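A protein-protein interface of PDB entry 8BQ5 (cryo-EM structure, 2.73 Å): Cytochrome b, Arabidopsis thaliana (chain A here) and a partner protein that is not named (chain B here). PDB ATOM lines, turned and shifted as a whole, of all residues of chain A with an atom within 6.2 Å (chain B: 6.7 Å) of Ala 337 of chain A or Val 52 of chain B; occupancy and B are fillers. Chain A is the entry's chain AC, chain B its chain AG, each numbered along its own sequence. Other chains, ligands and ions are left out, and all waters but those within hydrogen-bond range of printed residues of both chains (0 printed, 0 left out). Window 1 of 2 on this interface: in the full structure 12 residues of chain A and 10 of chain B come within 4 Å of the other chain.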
ATOM      1  N   PHE A 332      -2.284  28.505 -24.484  1.00  0.00           N
ATOM      2  CA  PHE A 332      -3.294  27.895 -25.342  1.00  0.00           C
ATOM      3  C   PHE A 332      -4.515  27.471 -24.538  1.00  0.00           C
ATOM      4  O   PHE A 332      -5.654  27.649 -24.984  1.00  0.00           O
ATOM      5  CB  PHE A 332      -2.700  26.699 -26.090  1.00  0.00           C
ATOM      6  CG  PHE A 332      -3.732  25.794 -26.704  1.00  0.00           C
ATOM      7  CD1 PHE A 332      -4.245  24.715 -26.000  1.00  0.00           C
ATOM      8  CD2 PHE A 332      -4.196  26.028 -27.986  1.00  0.00           C
ATOM      9  CE1 PHE A 332      -5.196  23.893 -26.562  1.00  0.00           C
ATOM     10  CE2 PHE A 332      -5.145  25.207 -28.554  1.00  0.00           C
ATOM     11  CZ  PHE A 332      -5.645  24.138 -27.842  1.00  0.00           C
ATOM     12  N   TRP A 333      -4.297  26.898 -23.354  1.00  0.00           N
ATOM     13  CA  TRP A 333      -5.415  26.427 -22.547  1.00  0.00           C
ATOM     14  C   TRP A 333      -6.210  27.594 -21.975  1.00  0.00           C
ATOM     15  O   TRP A 333      -7.421  27.478 -21.756  1.00  0.00           O
ATOM     16  CB  TRP A 333      -4.903  25.512 -21.436  1.00  0.00           C
ATOM     17  CG  TRP A 333      -4.428  24.199 -21.962  1.00  0.00           C
ATOM     18  CD1 TRP A 333      -3.160  23.704 -21.905  1.00  0.00           C
ATOM     19  CD2 TRP A 333      -5.214  23.212 -22.640  1.00  0.00           C
ATOM     20  NE1 TRP A 333      -3.105  22.470 -22.502  1.00  0.00           N
ATOM     21  CE2 TRP A 333      -4.354  22.144 -22.962  1.00  0.00           C
ATOM     22  CE3 TRP A 333      -6.560  23.126 -23.005  1.00  0.00           C
ATOM     23  CZ2 TRP A 333      -4.796  21.005 -23.629  1.00  0.00           C
ATOM     24  CZ3 TRP A 333      -6.997  21.995 -23.668  1.00  0.00           C
ATOM     25  CH2 TRP A 333      -6.118  20.950 -23.973  1.00  0.00           C
ATOM     26  N   LEU A 334      -5.545  28.722 -21.722  1.00  0.00           N
ATOM     27  CA  LEU A 334      -6.260  29.921 -21.302  1.00  0.00           C
ATOM     28  C   LEU A 334      -7.073  30.503 -22.451  1.00  0.00           C
ATOM     29  O   LEU A 334      -8.175  31.022 -22.242  1.00  0.00           O
ATOM     30  CB  LEU A 334      -5.275  30.955 -20.760  1.00  0.00           C
ATOM     31  CG  LEU A 334      -4.592  30.616 -19.435  1.00  0.00           C
ATOM     32  CD1 LEU A 334      -3.490  31.618 -19.140  1.00  0.00           C
ATOM     33  CD2 LEU A 334      -5.602  30.580 -18.301  1.00  0.00           C
ATOM     34  N   LEU A 335      -6.539  30.434 -23.673  1.00  0.00           N
ATOM     35  CA  LEU A 335      -7.285  30.905 -24.834  1.00  0.00           C
ATOM     36  C   LEU A 335      -8.514  30.042 -25.087  1.00  0.00           C
ATOM     37  O   LEU A 335      -9.582  30.556 -25.440  1.00  0.00           O
ATOM     38  CB  LEU A 335      -6.380  30.930 -26.066  1.00  0.00           C
ATOM     39  CG  LEU A 335      -7.068  31.127 -27.419  1.00  0.00           C
ATOM     40  CD1 LEU A 335      -7.566  32.554 -27.572  1.00  0.00           C
ATOM     41  CD2 LEU A 335      -6.132  30.756 -28.556  1.00  0.00           C
ATOM     42  N   LEU A 336      -8.383  28.723 -24.921  1.00  0.00           N
ATOM     43  CA  LEU A 336      -9.531  27.839 -25.086  1.00  0.00           C
ATOM     44  C   LEU A 336     -10.605  28.135 -24.046  1.00  0.00           C
ATOM     45  O   LEU A 336     -11.799  28.163 -24.360  1.00  0.00           O
ATOM     46  CB  LEU A 336      -9.087  26.378 -25.005  1.00  0.00           C
ATOM     47  CG  LEU A 336     -10.179  25.334 -25.251  1.00  0.00           C
ATOM     48  CD1 LEU A 336     -10.921  25.625 -26.543  1.00  0.00           C
ATOM     49  CD2 LEU A 336      -9.596  23.932 -25.269  1.00  0.00           C
ATOM     50  N   ALA A 337     -10.194  28.354 -22.795  1.00  0.00           N
ATOM     51  CA  ALA A 337     -11.153  28.712 -21.754  1.00  0.00           C
ATOM     52  C   ALA A 337     -11.792  30.062 -22.042  1.00  0.00           C
ATOM     53  O   ALA A 337     -12.968  30.285 -21.729  1.00  0.00           O
ATOM     54  CB  ALA A 337     -10.469  28.720 -20.388  1.00  0.00           C
ATOM     55  N   ASP A 338     -11.025  30.982 -22.628  1.00  0.00           N
ATOM     56  CA  ASP A 338     -11.562  32.292 -22.974  1.00  0.00           C
ATOM     57  C   ASP A 338     -12.596  32.194 -24.090  1.00  0.00           C
ATOM     58  O   ASP A 338     -13.633  32.868 -24.047  1.00  0.00           O
ATOM     59  CB  ASP A 338     -10.422  33.221 -23.379  1.00  0.00           C
ATOM     60  CG  ASP A 338     -10.755  34.673 -23.161  1.00  0.00           C
ATOM     61  OD1 ASP A 338     -11.448  34.987 -22.172  1.00  0.00           O
ATOM     62  OD2 ASP A 338     -10.320  35.500 -23.985  1.00  0.00           O
ATOM     63  N   CYS A 339     -12.328  31.367 -25.103  1.00  0.00           N
ATOM     64  CA  CYS A 339     -13.279  31.203 -26.197  1.00  0.00           C
ATOM     65  C   CYS A 339     -14.568  30.552 -25.712  1.00  0.00           C
ATOM     66  O   CYS A 339     -15.658  30.888 -26.190  1.00  0.00           O
ATOM     67  CB  CYS A 339     -12.649  30.386 -27.323  1.00  0.00           C
ATOM     68  SG  CYS A 339     -11.307  31.241 -28.179  1.00  0.00           S
ATOM     69  N   LEU A 340     -14.461  29.611 -24.773  1.00  0.00           N
ATOM     70  CA  LEU A 340     -15.653  29.047 -24.150  1.00  0.00           C
ATOM     71  C   LEU A 340     -16.432  30.118 -23.398  1.00  0.00           C
ATOM     72  O   LEU A 340     -17.665  30.162 -23.462  1.00  0.00           O
ATOM     73  CB  LEU A 340     -15.258  27.911 -23.207  1.00  0.00           C
ATOM     74  CG  LEU A 340     -14.712  26.630 -23.838  1.00  0.00           C
ATOM     75  CD1 LEU A 340     -14.595  25.529 -22.795  1.00  0.00           C
ATOM     76  CD2 LEU A 340     -15.585  26.178 -24.997  1.00  0.00           C
ATOM     77  N   LEU A 341     -15.723  30.991 -22.678  1.00  0.00           N
ATOM     78  CA  LEU A 341     -16.382  32.048 -21.916  1.00  0.00           C
ATOM     79  C   LEU A 341     -17.087  33.043 -22.829  1.00  0.00           C
ATOM     80  O   LEU A 341     -18.179  33.524 -22.507  1.00  0.00           O
ATOM     81  CB  LEU A 341     -15.361  32.767 -21.034  1.00  0.00           C
ATOM     82  CG  LEU A 341     -15.113  32.186 -19.642  1.00  0.00           C
ATOM     83  CD1 LEU A 341     -14.300  33.162 -18.811  1.00  0.00           C
ATOM     84  CD2 LEU A 341     -16.429  31.858 -18.955  1.00  0.00           C
ATOM     85  N   LEU A 342     -16.469  33.377 -23.965  1.00  0.00           N
ATOM     86  CA  LEU A 342     -17.082  34.334 -24.883  1.00  0.00           C
ATOM     87  C   LEU A 342     -18.388  33.795 -25.451  1.00  0.00           C
ATOM     88  O   LEU A 342     -19.370  34.536 -25.578  1.00  0.00           O
ATOM     89  CB  LEU A 342     -16.113  34.685 -26.011  1.00  0.00           C
ATOM     90  CG  LEU A 342     -15.045  35.733 -25.690  1.00  0.00           C
ATOM     91  CD1 LEU A 342     -13.972  35.739 -26.762  1.00  0.00           C
ATOM     92  CD2 LEU A 342     -15.657  37.114 -25.534  1.00  0.00           C
ATOM     93  N   LEU B  47      -5.723  25.234 -15.875  1.00  0.00           N
ATOM     94  CA  LEU B  47      -5.746  26.487 -16.622  1.00  0.00           C
ATOM     95  C   LEU B  47      -6.957  26.576 -17.540  1.00  0.00           C
ATOM     96  O   LEU B  47      -7.283  27.661 -18.033  1.00  0.00           O
ATOM     97  CB  LEU B  47      -4.455  26.641 -17.427  1.00  0.00           C
ATOM     98  CG  LEU B  47      -3.189  26.943 -16.624  1.00  0.00           C
ATOM     99  CD1 LEU B  47      -1.963  26.874 -17.516  1.00  0.00           C
ATOM    100  CD2 LEU B  47      -3.289  28.303 -15.959  1.00  0.00           C
ATOM    101  N   LEU B  48      -7.634  25.452 -17.782  1.00  0.00           N
ATOM    102  CA  LEU B  48      -8.812  25.461 -18.640  1.00  0.00           C
ATOM    103  C   LEU B  48     -10.101  25.515 -17.829  1.00  0.00           C
ATOM    104  O   LEU B  48     -11.045  26.220 -18.205  1.00  0.00           O
ATOM    105  CB  LEU B  48      -8.805  24.232 -19.548  1.00  0.00           C
ATOM    106  CG  LEU B  48     -10.108  23.908 -20.283  1.00  0.00           C
ATOM    107  CD1 LEU B  48     -10.372  24.921 -21.384  1.00  0.00           C
ATOM    108  CD2 LEU B  48     -10.067  22.501 -20.849  1.00  0.00           C
ATOM    109  N   VAL B  49     -10.157  24.794 -16.714  1.00  0.00           N
ATOM    110  CA  VAL B  49     -11.389  24.688 -15.938  1.00  0.00           C
ATOM    111  C   VAL B  49     -11.559  25.861 -14.979  1.00  0.00           C
ATOM    112  O   VAL B  49     -12.664  26.387 -14.830  1.00  0.00           O
ATOM    113  CB  VAL B  49     -11.420  23.338 -15.194  1.00  0.00           C
ATOM    114  CG1 VAL B  49     -12.610  23.273 -14.254  1.00  0.00           C
ATOM    115  CG2 VAL B  49     -11.468  22.192 -16.190  1.00  0.00           C
ATOM    116  N   THR B  50     -10.480  26.291 -14.324  1.00  0.00           N
ATOM    117  CA  THR B  50     -10.603  27.326 -13.298  1.00  0.00           C
ATOM    118  C   THR B  50     -11.171  28.639 -13.824  1.00  0.00           C
ATOM    119  O   THR B  50     -12.084  29.187 -13.182  1.00  0.00           O
ATOM    120  CB  THR B  50      -9.246  27.534 -12.614  1.00  0.00           C
ATOM    121  OG1 THR B  50      -8.929  26.384 -11.822  1.00  0.00           O
ATOM    122  CG2 THR B  50      -9.275  28.764 -11.719  1.00  0.00           C
ATOM    123  N   PRO B  51     -10.700  29.207 -14.946  1.00  0.00           N
ATOM    124  CA  PRO B  51     -11.324  30.455 -15.422  1.00  0.00           C
ATOM    125  C   PRO B  51     -12.797  30.307 -15.761  1.00  0.00           C
ATOM    126  O   PRO B  51     -13.578  31.235 -15.519  1.00  0.00           O
ATOM    127  CB  PRO B  51     -10.489  30.815 -16.658  1.00  0.00           C
ATOM    128  CG  PRO B  51      -9.204  30.104 -16.474  1.00  0.00           C
ATOM    129  CD  PRO B  51      -9.557  28.824 -15.794  1.00  0.00           C
ATOM    130  N   VAL B  52     -13.200  29.163 -16.317  1.00  0.00           N
ATOM    131  CA  VAL B  52     -14.602  28.965 -16.681  1.00  0.00           C
ATOM    132  C   VAL B  52     -15.467  28.849 -15.432  1.00  0.00           C
ATOM    133  O   VAL B  52     -16.528  29.475 -15.329  1.00  0.00           O
ATOM    134  CB  VAL B  52     -14.750  27.730 -17.588  1.00  0.00           C
ATOM    135  CG1 VAL B  52     -16.213  27.463 -17.882  1.00  0.00           C
ATOM    136  CG2 VAL B  52     -13.977  27.928 -18.879  1.00  0.00           C
ATOM    137  N   VAL B  53     -15.029  28.037 -14.467  1.00  0.00           N
ATOM    138  CA  VAL B  53     -15.811  27.842 -13.249  1.00  0.00           C
ATOM    139  C   VAL B  53     -15.781  29.097 -12.385  1.00  0.00           C
ATOM    140  O   VAL B  53     -16.802  29.495 -11.812  1.00  0.00           O
ATOM    141  CB  VAL B  53     -15.303  26.607 -12.486  1.00  0.00           C
ATOM    142  CG1 VAL B  53     -15.978  26.500 -11.124  1.00  0.00           C
ATOM    143  CG2 VAL B  53     -15.553  25.355 -13.303  1.00  0.00           C
ATOM    144  N   GLY B  54     -14.617  29.739 -12.279  1.00  0.00           N
ATOM    145  CA  GLY B  54     -14.525  30.953 -11.485  1.00  0.00           C
ATOM    146  C   GLY B  54     -15.384  32.075 -12.035  1.00  0.00           C
ATOM    147  O   GLY B  54     -16.035  32.802 -11.281  1.00  0.00           O
ATOM    148  N   THR B  55     -15.397  32.233 -13.359  1.00  0.00           N
ATOM    149  CA  THR B  55     -16.223  33.271 -13.966  1.00  0.00           C
ATOM    150  C   THR B  55     -17.704  32.931 -13.855  1.00  0.00           C
ATOM    151  O   THR B  55     -18.528  33.810 -13.575  1.00  0.00           O
ATOM    152  CB  THR B  55     -15.828  33.471 -15.429  1.00  0.00           C
ATOM    153  OG1 THR B  55     -14.420  33.719 -15.511  1.00  0.00           O
ATOM    154  CG2 THR B  55     -16.572  34.652 -16.023  1.00  0.00           C
ATOM    155  N   TYR B  56     -18.060  31.663 -14.069  1.00  0.00           N
ATOM    156  CA  TYR B  56     -19.456  31.255 -13.957  1.00  0.00           C
ATOM    157  C   TYR B  56     -19.971  31.445 -12.536  1.00  0.00           C
ATOM    158  O   TYR B  56     -21.074  31.962 -12.330  1.00  0.00           O
ATOM    159  CB  TYR B  56     -19.617  29.800 -14.397  1.00  0.00           C
ATOM    160  CG  TYR B  56     -21.054  29.328 -14.443  1.00  0.00           C
ATOM    161  CD1 TYR B  56     -21.830  29.517 -15.577  1.00  0.00           C
ATOM    162  CD2 TYR B  56     -21.632  28.694 -13.352  1.00  0.00           C
ATOM    163  CE1 TYR B  56     -23.141  29.087 -15.624  1.00  0.00           C
ATOM    164  CE2 TYR B  56     -22.942  28.262 -13.389  1.00  0.00           C
ATOM    165  CZ  TYR B  56     -23.692  28.460 -14.527  1.00  0.00           C
ATOM    166  OH  TYR B  56     -24.997  28.028 -14.568  1.00  0.00           O
ATOM    167  N   TRP B  57     -19.182  31.036 -11.540  1.00  0.00           N
ATOM    168  CA  TRP B  57     -19.615  31.191 -10.155  1.00  0.00           C
ATOM    169  C   TRP B  57     -19.767  32.659  -9.783  1.00  0.00           C
ATOM    170  O   TRP B  57     -20.712  33.033  -9.080  1.00  0.00           O
ATOM    171  CB  TRP B  57     -18.638  30.502  -9.201  1.00  0.00           C
ATOM    172  CG  TRP B  57     -18.685  31.089  -7.819  1.00  0.00           C
ATOM    173  CD1 TRP B  57     -19.509  30.713  -6.797  1.00  0.00           C
ATOM    174  CD2 TRP B  57     -17.877  32.159  -7.308  1.00  0.00           C
ATOM    175  NE1 TRP B  57     -19.268  31.485  -5.687  1.00  0.00           N
ATOM    176  CE2 TRP B  57     -18.273  32.380  -5.974  1.00  0.00           C
ATOM    177  CE3 TRP B  57     -16.862  32.954  -7.851  1.00  0.00           C
ATOM    178  CZ2 TRP B  57     -17.687  33.360  -5.176  1.00  0.00           C
ATOM    179  CZ3 TRP B  57     -16.285  33.928  -7.057  1.00  0.00           C
ATOM    180  CH2 TRP B  57     -16.699  34.122  -5.734  1.00  0.00           C
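O of Pro 51 of chain B is in hydrogen-bond range of OG1 of Thr 55 of chain B (2.6 Å).
Leu 47 of chain B touches Trp 333 of chain A.
Trp 333 of chain A touches Leu 48 of chain B.
CD2 of Leu 334 of chain A touches O of Leu 47 of chain B (3.4 Å).
Leu 48 of chain B touches Leu 336 of chain A (CD1 to CG, 3.9 Å).
Ala 337 of chain A touches Leu 48 of chain B (CB to O, 3.4 Å).
CG2 of Val 52 of chain B touches O of Ala 337 of chain A, 3.8 Å away.
Pro 51 of chain B touches Leu 341 of chain A (O to CD1, 3.9 Å).
Leu 341 of chain A touches Thr 55 of chain B.
Ala 337 of chain A touches two residues of chain B.
Printed residues of chain A within 4 Å of Pro 51 of chain B: Leu 341.
Val 52 of chain B touches just one residue of chain A: Ala 337.
Printed residues of chain A within 4 Å of Thr 55 of chain B: Leu 341.
The nearest residue of chain B that does not touch Ala 337 of chain A is Leu 47 of chain B (4.1 Å).
Hydrophobic or aromatic side chains of chain B that line the printed part of chain A: Leu 48 and Val 52.
Of the 11 printed residues of chain A, 5 touch a printed residue of chain B.
Hydrophobic or aromatic side chains of chain A that line the printed part of chain B: Leu 334, Leu 336, Ala 337 and Leu 341.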
